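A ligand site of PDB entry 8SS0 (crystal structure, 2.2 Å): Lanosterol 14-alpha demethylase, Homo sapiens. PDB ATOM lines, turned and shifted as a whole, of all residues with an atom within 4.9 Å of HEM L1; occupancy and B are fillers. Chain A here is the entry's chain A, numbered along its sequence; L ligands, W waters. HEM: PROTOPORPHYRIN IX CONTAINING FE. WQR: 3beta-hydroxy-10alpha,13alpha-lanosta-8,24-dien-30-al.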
ATOM      1  N   TYR A  82      -3.606  27.688 -41.301  1.00  0.00           N
ATOM      2  CA  TYR A  82      -3.992  28.580 -40.228  1.00  0.00           C
ATOM      3  C   TYR A  82      -4.552  29.909 -40.752  1.00  0.00           C
ATOM      4  O   TYR A  82      -5.340  30.561 -40.061  1.00  0.00           O
ATOM      5  CB  TYR A  82      -2.808  28.818 -39.285  1.00  0.00           C
ATOM      6  CG  TYR A  82      -2.505  27.726 -38.284  1.00  0.00           C
ATOM      7  CD1 TYR A  82      -3.383  26.683 -38.009  1.00  0.00           C
ATOM      8  CD2 TYR A  82      -1.311  27.760 -37.590  1.00  0.00           C
ATOM      9  CE1 TYR A  82      -3.059  25.694 -37.084  1.00  0.00           C
ATOM     10  CE2 TYR A  82      -0.977  26.799 -36.651  1.00  0.00           C
ATOM     11  CZ  TYR A  82      -1.861  25.758 -36.404  1.00  0.00           C
ATOM     12  OH  TYR A  82      -1.473  24.834 -35.473  1.00  0.00           O
ATOM     13  N   TYR A  96      -0.095  34.322 -39.998  1.00  0.00           N
ATOM     14  CA  TYR A  96      -0.198  33.369 -41.139  1.00  0.00           C
ATOM     15  C   TYR A  96      -0.673  34.032 -42.433  1.00  0.00           C
ATOM     16  O   TYR A  96      -0.910  33.305 -43.414  1.00  0.00           O
ATOM     17  CB  TYR A  96      -1.074  32.194 -40.686  1.00  0.00           C
ATOM     18  CG  TYR A  96      -0.625  31.605 -39.374  1.00  0.00           C
ATOM     19  CD1 TYR A  96       0.589  30.962 -39.263  1.00  0.00           C
ATOM     20  CD2 TYR A  96      -1.395  31.742 -38.232  1.00  0.00           C
ATOM     21  CE1 TYR A  96       1.017  30.431 -38.066  1.00  0.00           C
ATOM     22  CE2 TYR A  96      -0.976  31.223 -37.018  1.00  0.00           C
ATOM     23  CZ  TYR A  96       0.237  30.561 -36.929  1.00  0.00           C
ATOM     24  OH  TYR A  96       0.662  30.044 -35.731  1.00  0.00           O
ATOM     25  N   PHE A 103       6.815  36.552 -40.576  1.00  0.00           N
ATOM     26  CA  PHE A 103       6.193  36.187 -39.306  1.00  0.00           C
ATOM     27  C   PHE A 103       7.250  35.909 -38.230  1.00  0.00           C
ATOM     28  O   PHE A 103       6.979  36.185 -37.073  1.00  0.00           O
ATOM     29  CB  PHE A 103       5.280  34.969 -39.485  1.00  0.00           C
ATOM     30  CG  PHE A 103       4.696  34.395 -38.224  1.00  0.00           C
ATOM     31  CD1 PHE A 103       4.051  35.215 -37.319  1.00  0.00           C
ATOM     32  CD2 PHE A 103       4.802  33.041 -37.932  1.00  0.00           C
ATOM     33  CE1 PHE A 103       3.515  34.691 -36.144  1.00  0.00           C
ATOM     34  CE2 PHE A 103       4.264  32.517 -36.770  1.00  0.00           C
ATOM     35  CZ  PHE A 103       3.626  33.346 -35.873  1.00  0.00           C
ATOM     36  N   LYS A 107       7.636  37.768 -34.670  1.00  0.00           N
ATOM     37  CA  LYS A 107       7.704  36.942 -33.469  1.00  0.00           C
ATOM     38  C   LYS A 107       8.776  37.474 -32.518  1.00  0.00           C
ATOM     39  O   LYS A 107       8.576  37.466 -31.310  1.00  0.00           O
ATOM     40  CB  LYS A 107       8.000  35.495 -33.890  1.00  0.00           C
ATOM     41  CG  LYS A 107       7.301  34.376 -33.129  1.00  0.00           C
ATOM     42  CD  LYS A 107       7.631  33.016 -33.732  1.00  0.00           C
ATOM     43  CE  LYS A 107       7.526  31.889 -32.734  1.00  0.00           C
ATOM     44  NZ  LYS A 107       8.037  30.624 -33.288  1.00  0.00           N
ATOM     45  N   LEU A 114       9.341  40.217 -23.101  1.00  0.00           N
ATOM     46  CA  LEU A 114       9.116  38.979 -22.368  1.00  0.00           C
ATOM     47  C   LEU A 114      10.437  38.488 -21.776  1.00  0.00           C
ATOM     48  O   LEU A 114      11.121  37.679 -22.377  1.00  0.00           O
ATOM     49  CB  LEU A 114       8.541  37.922 -23.317  1.00  0.00           C
ATOM     50  CG  LEU A 114       7.208  38.254 -23.984  1.00  0.00           C
ATOM     51  CD1 LEU A 114       6.813  37.180 -24.971  1.00  0.00           C
ATOM     52  CD2 LEU A 114       6.116  38.420 -22.945  1.00  0.00           C
ATOM     53  N   LEU A 161       1.405  43.561 -21.235  1.00  0.00           N
ATOM     54  CA  LEU A 161       2.041  43.371 -22.520  1.00  0.00           C
ATOM     55  C   LEU A 161       1.949  44.645 -23.364  1.00  0.00           C
ATOM     56  O   LEU A 161       2.843  44.911 -24.163  1.00  0.00           O
ATOM     57  CB  LEU A 161       1.378  42.197 -23.270  1.00  0.00           C
ATOM     58  CG  LEU A 161       1.365  40.821 -22.607  1.00  0.00           C
ATOM     59  CD1 LEU A 161       0.594  39.816 -23.467  1.00  0.00           C
ATOM     60  CD2 LEU A 161       2.753  40.269 -22.337  1.00  0.00           C
ATOM     61  N   LEU A 259      -1.343  40.072 -30.003  1.00  0.00           N
ATOM     62  CA  LEU A 259      -0.666  40.020 -28.707  1.00  0.00           C
ATOM     63  C   LEU A 259      -1.692  39.927 -27.572  1.00  0.00           C
ATOM     64  O   LEU A 259      -1.488  39.184 -26.611  1.00  0.00           O
ATOM     65  CB  LEU A 259       0.225  41.261 -28.572  1.00  0.00           C
ATOM     66  CG  LEU A 259       0.995  41.383 -27.262  1.00  0.00           C
ATOM     67  CD1 LEU A 259       2.003  40.244 -27.093  1.00  0.00           C
ATOM     68  CD2 LEU A 259       1.690  42.725 -27.158  1.00  0.00           C
ATOM     69  N   ALA A 262      -3.300  36.549 -27.603  1.00  0.00           N
ATOM     70  CA  ALA A 262      -2.257  35.644 -27.149  1.00  0.00           C
ATOM     71  C   ALA A 262      -2.234  35.603 -25.614  1.00  0.00           C
ATOM     72  O   ALA A 262      -2.160  34.517 -25.035  1.00  0.00           O
ATOM     73  CB  ALA A 262      -0.929  36.070 -27.722  1.00  0.00           C
ATOM     74  N   GLY A 263      -2.331  36.791 -25.000  1.00  0.00           N
ATOM     75  CA  GLY A 263      -2.236  36.925 -23.554  1.00  0.00           C
ATOM     76  C   GLY A 263      -3.499  36.477 -22.822  1.00  0.00           C
ATOM     77  O   GLY A 263      -3.413  36.262 -21.617  1.00  0.00           O
ATOM     78  N   THR A 266      -6.092  31.777 -24.242  1.00  0.00           N
ATOM     79  CA  THR A 266      -5.565  30.530 -23.719  1.00  0.00           C
ATOM     80  C   THR A 266      -5.475  30.598 -22.190  1.00  0.00           C
ATOM     81  O   THR A 266      -5.640  29.582 -21.519  1.00  0.00           O
ATOM     82  CB  THR A 266      -4.246  30.194 -24.419  1.00  0.00           C
ATOM     83  OG1 THR A 266      -3.469  31.390 -24.473  1.00  0.00           O
ATOM     84  CG2 THR A 266      -4.447  29.693 -25.832  1.00  0.00           C
ATOM     85  N   SER A 267      -5.246  31.789 -21.644  1.00  0.00           N
ATOM     86  CA  SER A 267      -5.012  31.921 -20.221  1.00  0.00           C
ATOM     87  C   SER A 267      -6.315  31.842 -19.432  1.00  0.00           C
ATOM     88  O   SER A 267      -6.366  31.264 -18.340  1.00  0.00           O
ATOM     89  CB  SER A 267      -4.273  33.190 -19.900  1.00  0.00           C
ATOM     90  OG  SER A 267      -2.861  32.981 -19.885  1.00  0.00           O
ATOM     91  N   THR A 270      -7.748  28.249 -19.305  1.00  0.00           N
ATOM     92  CA  THR A 270      -6.867  27.489 -18.423  1.00  0.00           C
ATOM     93  C   THR A 270      -7.100  27.867 -16.948  1.00  0.00           C
ATOM     94  O   THR A 270      -7.161  26.986 -16.072  1.00  0.00           O
ATOM     95  CB  THR A 270      -5.379  27.710 -18.755  1.00  0.00           C
ATOM     96  OG1 THR A 270      -5.183  27.420 -20.143  1.00  0.00           O
ATOM     97  CG2 THR A 270      -4.469  26.863 -17.892  1.00  0.00           C
ATOM     98  N   LEU A 322      -3.056  22.137 -17.721  1.00  0.00           N
ATOM     99  CA  LEU A 322      -2.731  22.215 -19.131  1.00  0.00           C
ATOM    100  C   LEU A 322      -2.638  20.810 -19.716  1.00  0.00           C
ATOM    101  O   LEU A 322      -2.790  20.616 -20.922  1.00  0.00           O
ATOM    102  CB  LEU A 322      -1.433  23.005 -19.288  1.00  0.00           C
ATOM    103  CG  LEU A 322      -1.602  24.525 -19.164  1.00  0.00           C
ATOM    104  CD1 LEU A 322      -0.288  25.194 -18.811  1.00  0.00           C
ATOM    105  CD2 LEU A 322      -2.118  25.111 -20.454  1.00  0.00           C
ATOM    106  N   PRO A 327      -5.655  24.537 -23.730  1.00  0.00           N
ATOM    107  CA  PRO A 327      -6.504  25.460 -24.492  1.00  0.00           C
ATOM    108  C   PRO A 327      -6.397  25.212 -25.988  1.00  0.00           C
ATOM    109  O   PRO A 327      -7.298  25.597 -26.720  1.00  0.00           O
ATOM    110  CB  PRO A 327      -5.942  26.836 -24.104  1.00  0.00           C
ATOM    111  CG  PRO A 327      -4.497  26.557 -23.768  1.00  0.00           C
ATOM    112  CD  PRO A 327      -4.538  25.216 -23.068  1.00  0.00           C
ATOM    113  N   ILE A 328      -5.298  24.558 -26.411  1.00  0.00           N
ATOM    114  CA  ILE A 328      -5.076  24.208 -27.816  1.00  0.00           C
ATOM    115  C   ILE A 328      -5.065  22.685 -27.965  1.00  0.00           C
ATOM    116  O   ILE A 328      -4.112  22.006 -27.592  1.00  0.00           O
ATOM    117  CB  ILE A 328      -3.828  24.923 -28.381  1.00  0.00           C
ATOM    118  CG1 ILE A 328      -4.157  26.387 -28.683  1.00  0.00           C
ATOM    119  CG2 ILE A 328      -3.293  24.215 -29.609  1.00  0.00           C
ATOM    120  CD1 ILE A 328      -2.995  27.271 -29.095  1.00  0.00           C
ATOM    121  N   MET A 331      -2.952  20.913 -33.390  1.00  0.00           N
ATOM    122  CA  MET A 331      -2.099  21.806 -34.207  1.00  0.00           C
ATOM    123  C   MET A 331      -2.125  21.220 -35.628  1.00  0.00           C
ATOM    124  O   MET A 331      -2.218  20.008 -35.718  1.00  0.00           O
ATOM    125  CB  MET A 331      -0.692  21.945 -33.659  1.00  0.00           C
ATOM    126  CG  MET A 331      -0.654  22.665 -32.340  1.00  0.00           C
ATOM    127  SD  MET A 331       1.046  22.860 -31.785  1.00  0.00           S
ATOM    128  CE  MET A 331       1.393  21.208 -31.217  1.00  0.00           C
ATOM    129  N   ARG A 333      -0.848  21.313 -39.945  1.00  0.00           N
ATOM    130  CA  ARG A 333       0.074  21.659 -41.012  1.00  0.00           C
ATOM    131  C   ARG A 333      -0.438  21.058 -42.303  1.00  0.00           C
ATOM    132  O   ARG A 333      -1.177  20.070 -42.270  1.00  0.00           O
ATOM    133  CB  ARG A 333       1.472  21.109 -40.744  1.00  0.00           C
ATOM    134  CG  ARG A 333       2.058  21.543 -39.409  1.00  0.00           C
ATOM    135  CD  ARG A 333       2.407  23.023 -39.396  1.00  0.00           C
ATOM    136  NE  ARG A 333       3.196  23.346 -38.205  1.00  0.00           N
ATOM    137  CZ  ARG A 333       2.707  23.619 -37.004  1.00  0.00           C
ATOM    138  NH1 ARG A 333       1.401  23.734 -36.815  1.00  0.00           N
ATOM    139  NH2 ARG A 333       3.527  23.821 -36.002  1.00  0.00           N
ATOM    140  N   VAL A 391       2.757  18.576 -24.596  1.00  0.00           N
ATOM    141  CA  VAL A 391       3.131  19.610 -25.548  1.00  0.00           C
ATOM    142  C   VAL A 391       2.097  20.728 -25.605  1.00  0.00           C
ATOM    143  O   VAL A 391       1.849  21.254 -26.681  1.00  0.00           O
ATOM    144  CB  VAL A 391       3.349  19.008 -26.949  1.00  0.00           C
ATOM    145  CG1 VAL A 391       4.692  18.290 -27.073  1.00  0.00           C
ATOM    146  CG2 VAL A 391       2.208  18.078 -27.342  1.00  0.00           C
ATOM    147  N   PRO A 392       1.568  21.216 -24.452  1.00  0.00           N
ATOM    148  CA  PRO A 392       0.496  22.218 -24.473  1.00  0.00           C
ATOM    149  C   PRO A 392       0.926  23.547 -25.089  1.00  0.00           C
ATOM    150  O   PRO A 392       0.077  24.263 -25.634  1.00  0.00           O
ATOM    151  CB  PRO A 392       0.140  22.373 -22.996  1.00  0.00           C
ATOM    152  CG  PRO A 392       1.436  22.081 -22.282  1.00  0.00           C
ATOM    153  CD  PRO A 392       2.024  20.943 -23.082  1.00  0.00           C
ATOM    154  N   PHE A 393       2.239  23.822 -25.019  1.00  0.00           N
ATOM    155  CA  PHE A 393       2.855  24.983 -25.650  1.00  0.00           C
ATOM    156  C   PHE A 393       3.647  24.601 -26.902  1.00  0.00           C
ATOM    157  O   PHE A 393       4.356  25.456 -27.438  1.00  0.00           O
ATOM    158  CB  PHE A 393       3.805  25.683 -24.676  1.00  0.00           C
ATOM    159  CG  PHE A 393       3.122  26.285 -23.489  1.00  0.00           C
ATOM    160  CD1 PHE A 393       2.589  27.564 -23.552  1.00  0.00           C
ATOM    161  CD2 PHE A 393       2.950  25.557 -22.340  1.00  0.00           C
ATOM    162  CE1 PHE A 393       1.919  28.091 -22.461  1.00  0.00           C
ATOM    163  CE2 PHE A 393       2.290  26.085 -21.250  1.00  0.00           C
ATOM    164  CZ  PHE A 393       1.768  27.352 -21.317  1.00  0.00           C
ATOM    165  N   GLY A 394       3.501  23.357 -27.382  1.00  0.00           N
ATOM    166  CA  GLY A 394       4.052  22.970 -28.663  1.00  0.00           C
ATOM    167  C   GLY A 394       5.505  22.528 -28.558  1.00  0.00           C
ATOM    168  O   GLY A 394       5.927  22.145 -27.486  1.00  0.00           O
ATOM    169  N   ARG A 397       9.946  24.690 -34.483  1.00  0.00           N
ATOM    170  CA  ARG A 397      10.045  26.052 -35.035  1.00  0.00           C
ATOM    171  C   ARG A 397       8.778  26.871 -34.818  1.00  0.00           C
ATOM    172  O   ARG A 397       8.780  28.078 -35.085  1.00  0.00           O
ATOM    173  CB  ARG A 397      10.289  26.044 -36.550  1.00  0.00           C
ATOM    174  CG  ARG A 397      11.705  25.700 -36.973  1.00  0.00           C
ATOM    175  CD  ARG A 397      11.837  25.420 -38.470  1.00  0.00           C
ATOM    176  NE  ARG A 397      13.156  24.945 -38.854  1.00  0.00           N
ATOM    177  CZ  ARG A 397      13.643  23.729 -38.617  1.00  0.00           C
ATOM    178  NH1 ARG A 397      13.028  22.894 -37.802  1.00  0.00           N
ATOM    179  NH2 ARG A 397      14.765  23.330 -39.207  1.00  0.00           N
ATOM    180  N   HIS A 398       7.689  26.230 -34.382  1.00  0.00           N
ATOM    181  CA  HIS A 398       6.418  26.928 -34.326  1.00  0.00           C
ATOM    182  C   HIS A 398       5.960  27.161 -32.894  1.00  0.00           C
ATOM    183  O   HIS A 398       4.857  27.660 -32.706  1.00  0.00           O
ATOM    184  CB  HIS A 398       5.371  26.167 -35.161  1.00  0.00           C
ATOM    185  CG  HIS A 398       5.407  26.452 -36.633  1.00  0.00           C
ATOM    186  ND1 HIS A 398       5.070  27.698 -37.130  1.00  0.00           N
ATOM    187  CD2 HIS A 398       5.707  25.677 -37.693  1.00  0.00           C
ATOM    188  CE1 HIS A 398       5.180  27.677 -38.452  1.00  0.00           C
ATOM    189  NE2 HIS A 398       5.556  26.457 -38.822  1.00  0.00           N
ATOM    190  N   ARG A 399       6.811  26.845 -31.901  1.00  0.00           N
ATOM    191  CA  ARG A 399       6.365  26.712 -30.513  1.00  0.00           C
ATOM    192  C   ARG A 399       6.171  28.094 -29.886  1.00  0.00           C
ATOM    193  O   ARG A 399       6.525  29.105 -30.489  1.00  0.00           O
ATOM    194  CB  ARG A 399       7.340  25.875 -29.677  1.00  0.00           C
ATOM    195  CG  ARG A 399       8.492  26.665 -29.072  1.00  0.00           C
ATOM    196  CD  ARG A 399       9.749  25.814 -29.050  1.00  0.00           C
ATOM    197  NE  ARG A 399      10.986  26.551 -28.829  1.00  0.00           N
ATOM    198  CZ  ARG A 399      11.915  26.834 -29.749  1.00  0.00           C
ATOM    199  NH1 ARG A 399      11.657  26.758 -31.048  1.00  0.00           N
ATOM    200  NH2 ARG A 399      13.107  27.256 -29.360  1.00  0.00           N
ATOM    201  N   CYS A 400       5.594  28.075 -28.666  1.00  0.00           N
ATOM    202  CA  CYS A 400       5.063  29.256 -28.012  1.00  0.00           C
ATOM    203  C   CYS A 400       6.217  30.088 -27.469  1.00  0.00           C
ATOM    204  O   CYS A 400       7.078  29.539 -26.792  1.00  0.00           O
ATOM    205  CB  CYS A 400       4.151  28.902 -26.847  1.00  0.00           C
ATOM    206  SG  CYS A 400       3.045  30.247 -26.329  1.00  0.00           S
ATOM    207  N   ILE A 401       6.185  31.391 -27.737  1.00  0.00           N
ATOM    208  CA  ILE A 401       7.108  32.332 -27.138  1.00  0.00           C
ATOM    209  C   ILE A 401       6.632  32.775 -25.753  1.00  0.00           C
ATOM    210  O   ILE A 401       7.358  33.459 -25.037  1.00  0.00           O
ATOM    211  CB  ILE A 401       7.318  33.558 -28.057  1.00  0.00           C
ATOM    212  CG1 ILE A 401       6.063  34.424 -28.158  1.00  0.00           C
ATOM    213  CG2 ILE A 401       7.811  33.100 -29.417  1.00  0.00           C
ATOM    214  CD1 ILE A 401       6.171  35.590 -29.110  1.00  0.00           C
ATOM    215  N   GLY A 402       5.395  32.431 -25.388  1.00  0.00           N
ATOM    216  CA  GLY A 402       4.689  33.158 -24.333  1.00  0.00           C
ATOM    217  C   GLY A 402       4.408  32.307 -23.097  1.00  0.00           C
ATOM    218  O   GLY A 402       3.669  32.738 -22.208  1.00  0.00           O
ATOM    219  N   PHE A 405       5.453  34.280 -19.659  1.00  0.00           N
ATOM    220  CA  PHE A 405       4.436  35.253 -19.317  1.00  0.00           C
ATOM    221  C   PHE A 405       3.151  34.593 -18.849  1.00  0.00           C
ATOM    222  O   PHE A 405       2.544  35.010 -17.880  1.00  0.00           O
ATOM    223  CB  PHE A 405       4.055  36.125 -20.507  1.00  0.00           C
ATOM    224  CG  PHE A 405       2.927  37.047 -20.138  1.00  0.00           C
ATOM    225  CD1 PHE A 405       3.154  38.113 -19.275  1.00  0.00           C
ATOM    226  CD2 PHE A 405       1.640  36.772 -20.540  1.00  0.00           C
ATOM    227  CE1 PHE A 405       2.098  38.927 -18.886  1.00  0.00           C
ATOM    228  CE2 PHE A 405       0.586  37.603 -20.178  1.00  0.00           C
ATOM    229  CZ  PHE A 405       0.827  38.674 -19.347  1.00  0.00           C
ATOM    230  N   ALA A 406       2.714  33.568 -19.600  1.00  0.00           N
ATOM    231  CA  ALA A 406       1.495  32.820 -19.326  1.00  0.00           C
ATOM    232  C   ALA A 406       1.515  32.288 -17.899  1.00  0.00           C
ATOM    233  O   ALA A 406       0.498  32.382 -17.200  1.00  0.00           O
ATOM    234  CB  ALA A 406       1.352  31.691 -20.327  1.00  0.00           C
ATOM    235  N   ILE A 410      -0.962  33.452 -14.679  1.00  0.00           N
ATOM    236  CA  ILE A 410      -1.867  32.494 -14.067  1.00  0.00           C
ATOM    237  C   ILE A 410      -1.467  32.215 -12.621  1.00  0.00           C
ATOM    238  O   ILE A 410      -2.336  32.075 -11.760  1.00  0.00           O
ATOM    239  CB  ILE A 410      -1.911  31.214 -14.933  1.00  0.00           C
ATOM    240  CG1 ILE A 410      -2.441  31.531 -16.334  1.00  0.00           C
ATOM    241  CG2 ILE A 410      -2.734  30.138 -14.252  1.00  0.00           C
ATOM    242  CD1 ILE A 410      -2.176  30.462 -17.365  1.00  0.00           C
HETATM  243  CHA HEM L   1       2.377  29.219 -30.457  1.00  0.00           C
HETATM  244  CHB HEM L   1      -0.040  27.497 -26.714  1.00  0.00           C
HETATM  245  CHC HEM L   1       0.119  31.836 -24.491  1.00  0.00           C
HETATM  246  CHD HEM L   1       2.237  33.621 -28.449  1.00  0.00           C
HETATM  247  C1A HEM L   1       1.715  28.390 -29.618  1.00  0.00           C
HETATM  248  C2A HEM L   1       1.509  27.036 -29.854  1.00  0.00           C
HETATM  249  C3A HEM L   1       0.854  26.537 -28.797  1.00  0.00           C
HETATM  250  C4A HEM L   1       0.624  27.589 -27.912  1.00  0.00           C
HETATM  251  CMA HEM L   1       0.398  25.122 -28.580  1.00  0.00           C
HETATM  252  CAA HEM L   1       1.975  26.253 -31.067  1.00  0.00           C
HETATM  253  CBA HEM L   1       1.243  26.566 -32.397  1.00  0.00           C
HETATM  254  CGA HEM L   1       1.600  25.544 -33.502  1.00  0.00           C
HETATM  255  O1A HEM L   1       0.951  25.472 -34.588  1.00  0.00           O
HETATM  256  O2A HEM L   1       2.542  24.713 -33.340  1.00  0.00           O
HETATM  257  C1B HEM L   1      -0.166  28.567 -25.813  1.00  0.00           C
HETATM  258  C2B HEM L   1      -0.719  28.368 -24.546  1.00  0.00           C
HETATM  259  C3B HEM L   1      -0.690  29.569 -23.914  1.00  0.00           C
HETATM  260  C4B HEM L   1      -0.084  30.515 -24.848  1.00  0.00           C
HETATM  261  CMB HEM L   1      -1.254  27.092 -23.954  1.00  0.00           C
HETATM  262  CAB HEM L   1      -1.110  29.909 -22.577  1.00  0.00           C
HETATM  263  CBB HEM L   1      -1.504  28.980 -21.700  1.00  0.00           C
HETATM  264  C1C HEM L   1       0.741  32.698 -25.355  1.00  0.00           C
HETATM  265  C2C HEM L   1       1.178  33.994 -25.034  1.00  0.00           C
HETATM  266  C3C HEM L   1       1.781  34.496 -26.196  1.00  0.00           C
HETATM  267  C4C HEM L   1       1.705  33.489 -27.188  1.00  0.00           C
HETATM  268  CMC HEM L   1       1.023  34.703 -23.704  1.00  0.00           C
HETATM  269  CAC HEM L   1       2.441  35.799 -26.399  1.00  0.00           C
HETATM  270  CBC HEM L   1       2.775  36.607 -25.390  1.00  0.00           C
HETATM  271  C1D HEM L   1       2.444  32.538 -29.266  1.00  0.00           C
HETATM  272  C2D HEM L   1       3.205  32.675 -30.510  1.00  0.00           C
HETATM  273  C3D HEM L   1       3.267  31.463 -31.060  1.00  0.00           C
HETATM  274  C4D HEM L   1       2.536  30.568 -30.146  1.00  0.00           C
HETATM  275  CMD HEM L   1       3.843  33.925 -31.074  1.00  0.00           C
HETATM  276  CAD HEM L   1       4.014  31.156 -32.333  1.00  0.00           C
HETATM  277  CBD HEM L   1       3.211  30.504 -33.465  1.00  0.00           C
HETATM  278  CGD HEM L   1       4.091  30.029 -34.604  1.00  0.00           C
HETATM  279  O1D HEM L   1       3.499  29.494 -35.576  1.00  0.00           O
HETATM  280  O2D HEM L   1       5.354  30.152 -34.585  1.00  0.00           O
HETATM  281  NA  HEM L   1       1.164  28.735 -28.420  1.00  0.00           N
HETATM  282  NB  HEM L   1       0.193  29.827 -25.956  1.00  0.00           N
HETATM  283  NC  HEM L   1       1.059  32.399 -26.654  1.00  0.00           N
HETATM  284  ND  HEM L   1       2.068  31.274 -29.106  1.00  0.00           N
HETATM  285 FE   HEM L   1       1.085  30.583 -27.660  1.00  0.00          FE
HETATM  286  C2  WQR L   2      -4.111  28.968 -34.568  1.00  0.00           C
HETATM  287  C1  WQR L   2      -3.822  28.393 -33.164  1.00  0.00           C
HETATM  288  C31 WQR L   2      -3.191  27.016 -33.302  1.00  0.00           C
HETATM  289  C30 WQR L   2      -4.231  26.011 -33.758  1.00  0.00           C
HETATM  290  C28 WQR L   2      -5.334  25.869 -32.733  1.00  0.00           C
HETATM  291  O29 WQR L   2      -6.204  24.829 -33.133  1.00  0.00           O
HETATM  292  C25 WQR L   2      -6.113  27.166 -32.620  1.00  0.00           C
HETATM  293  C26 WQR L   2      -6.930  27.441 -33.885  1.00  0.00           C
HETATM  294  C27 WQR L   2      -7.102  27.040 -31.473  1.00  0.00           C
HETATM  295  C3  WQR L   2      -5.073  28.285 -32.236  1.00  0.00           C
HETATM  296  C4  WQR L   2      -5.684  29.656 -32.160  1.00  0.00           C
HETATM  297  C5  WQR L   2      -4.717  30.448 -31.291  1.00  0.00           C
HETATM  298  C6  WQR L   2      -3.376  30.268 -31.665  1.00  0.00           C
HETATM  299  C24 WQR L   2      -2.940  29.272 -32.561  1.00  0.00           C
HETATM  300  C23 WQR L   2      -1.603  29.152 -32.959  1.00  0.00           C
HETATM  301  C22 WQR L   2      -0.764  30.440 -32.795  1.00  0.00           C
HETATM  302  C10 WQR L   2      -1.548  31.645 -32.260  1.00  0.00           C
HETATM  303  C11 WQR L   2      -2.390  32.330 -33.359  1.00  0.00           C
HETATM  304  C7  WQR L   2      -2.429  31.162 -31.133  1.00  0.00           C
HETATM  305  C8  WQR L   2      -1.657  30.589 -30.098  1.00  0.00           C
HETATM  306  O32 WQR L   2      -2.036  30.543 -28.935  1.00  0.00           O
HETATM  307  C9  WQR L   2      -2.992  32.457 -30.667  1.00  0.00           C
HETATM  308  C21 WQR L   2      -1.706  33.289 -30.543  1.00  0.00           C
HETATM  309  C12 WQR L   2      -0.708  32.692 -31.535  1.00  0.00           C
HETATM  310  C13 WQR L   2      -0.257  33.824 -32.445  1.00  0.00           C
HETATM  311  C20 WQR L   2       0.961  33.425 -33.280  1.00  0.00           C
HETATM  312  C14 WQR L   2       0.123  35.008 -31.562  1.00  0.00           C
HETATM  313  C15 WQR L   2       0.834  36.092 -32.386  1.00  0.00           C
HETATM  314  C16 WQR L   2      -0.197  36.914 -33.153  1.00  0.00           C
HETATM  315  C17 WQR L   2       0.431  38.203 -33.684  1.00  0.00           C
HETATM  316  C19 WQR L   2      -0.491  38.828 -34.712  1.00  0.00           C
HETATM  317  C18 WQR L   2       1.772  37.902 -34.349  1.00  0.00           C
HETATM  318  O   HOH W   1      -2.523  33.267 -22.739  1.00  0.00           O
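SG of Cys 400 is bound to FE of HEM L1 (2.4 Å).
A ring nitrogen (ND1) of His 398 is in hydrogen-bond range of an oxygen (O1D) of HEM L1 (2.8 Å).
The side-chain hydroxyl (OH) of Tyr 82 sits at hydrogen-bond distance from an oxygen (O1A) of HEM L1.
The guanidinium group (NH1) of Arg 333 lies within salt-bridge range of an oxygen (O1A) of HEM L1 (2.9 Å).
The side-chain amino group of Lys 107 lies within salt-bridge range of an oxygen (O2D) of HEM L1 (3.0 Å).
The side-chain hydroxyl of Tyr 96 sits at hydrogen-bond distance from an oxygen (O1D) of HEM L1, 2.9 Å away.
O2A of HEM L1 sits close to SD of Met 331, at 2.8 Å.
OH of Tyr 82 is in hydrogen-bond range of NH1 of Arg 333 (3.4 Å).
O of Thr 266 lies within hydrogen-bond range of OG1 of Thr 270 (2.6 Å).
The backbone NH of Cys 400 is in hydrogen-bond range of the backbone carbonyl oxygen of Phe 393, at 3.1 Å.
OG1 of Thr 266 is in hydrogen-bond range of O of Ala 262 (3.4 Å).
NZ of Lys 107 is in hydrogen-bond range of O of Arg 397, 3.2 Å away.
The side-chain sulfur (SG) of Cys 400 sits close to the backbone NH (N) of Gly 402.
Residues that only touch HEM L1: Phe 103 (3.3 Å), Ala 262 (3.4 Å), Gly 263 (3.9 Å), Thr 266 (3.4 Å), Pro 327 (3.3 Å), Ile 328 (3.8 Å), Pro 392 (3.1 Å), Phe 393 (3.3 Å), Gly 394 (3.8 Å), Arg 399 (3.7 Å), Ile 401 (3.5 Å), Gly 402 (3.6 Å), Phe 405 (3.8 Å) and Ala 406 (3.8 Å).
Hydrophobic or aromatic side chains within 4 Å of HEM L1: Tyr 82, Tyr 96, Phe 103, Ala 262, Pro 327, Ile 328, Met 331, Phe 393, His 398, Ile 401, Phe 405 and Ala 406.
Of the 30 residues printed, 21 come within 4 Å of HEM L1.
Water W1 lies within hydrogen-bond range of O of Ala 262 (2.6 Å), OG1 of Thr 266 (2.7 Å), OG of Ser 267 (2.9 Å) and O of Gly 263 (3.3 Å).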
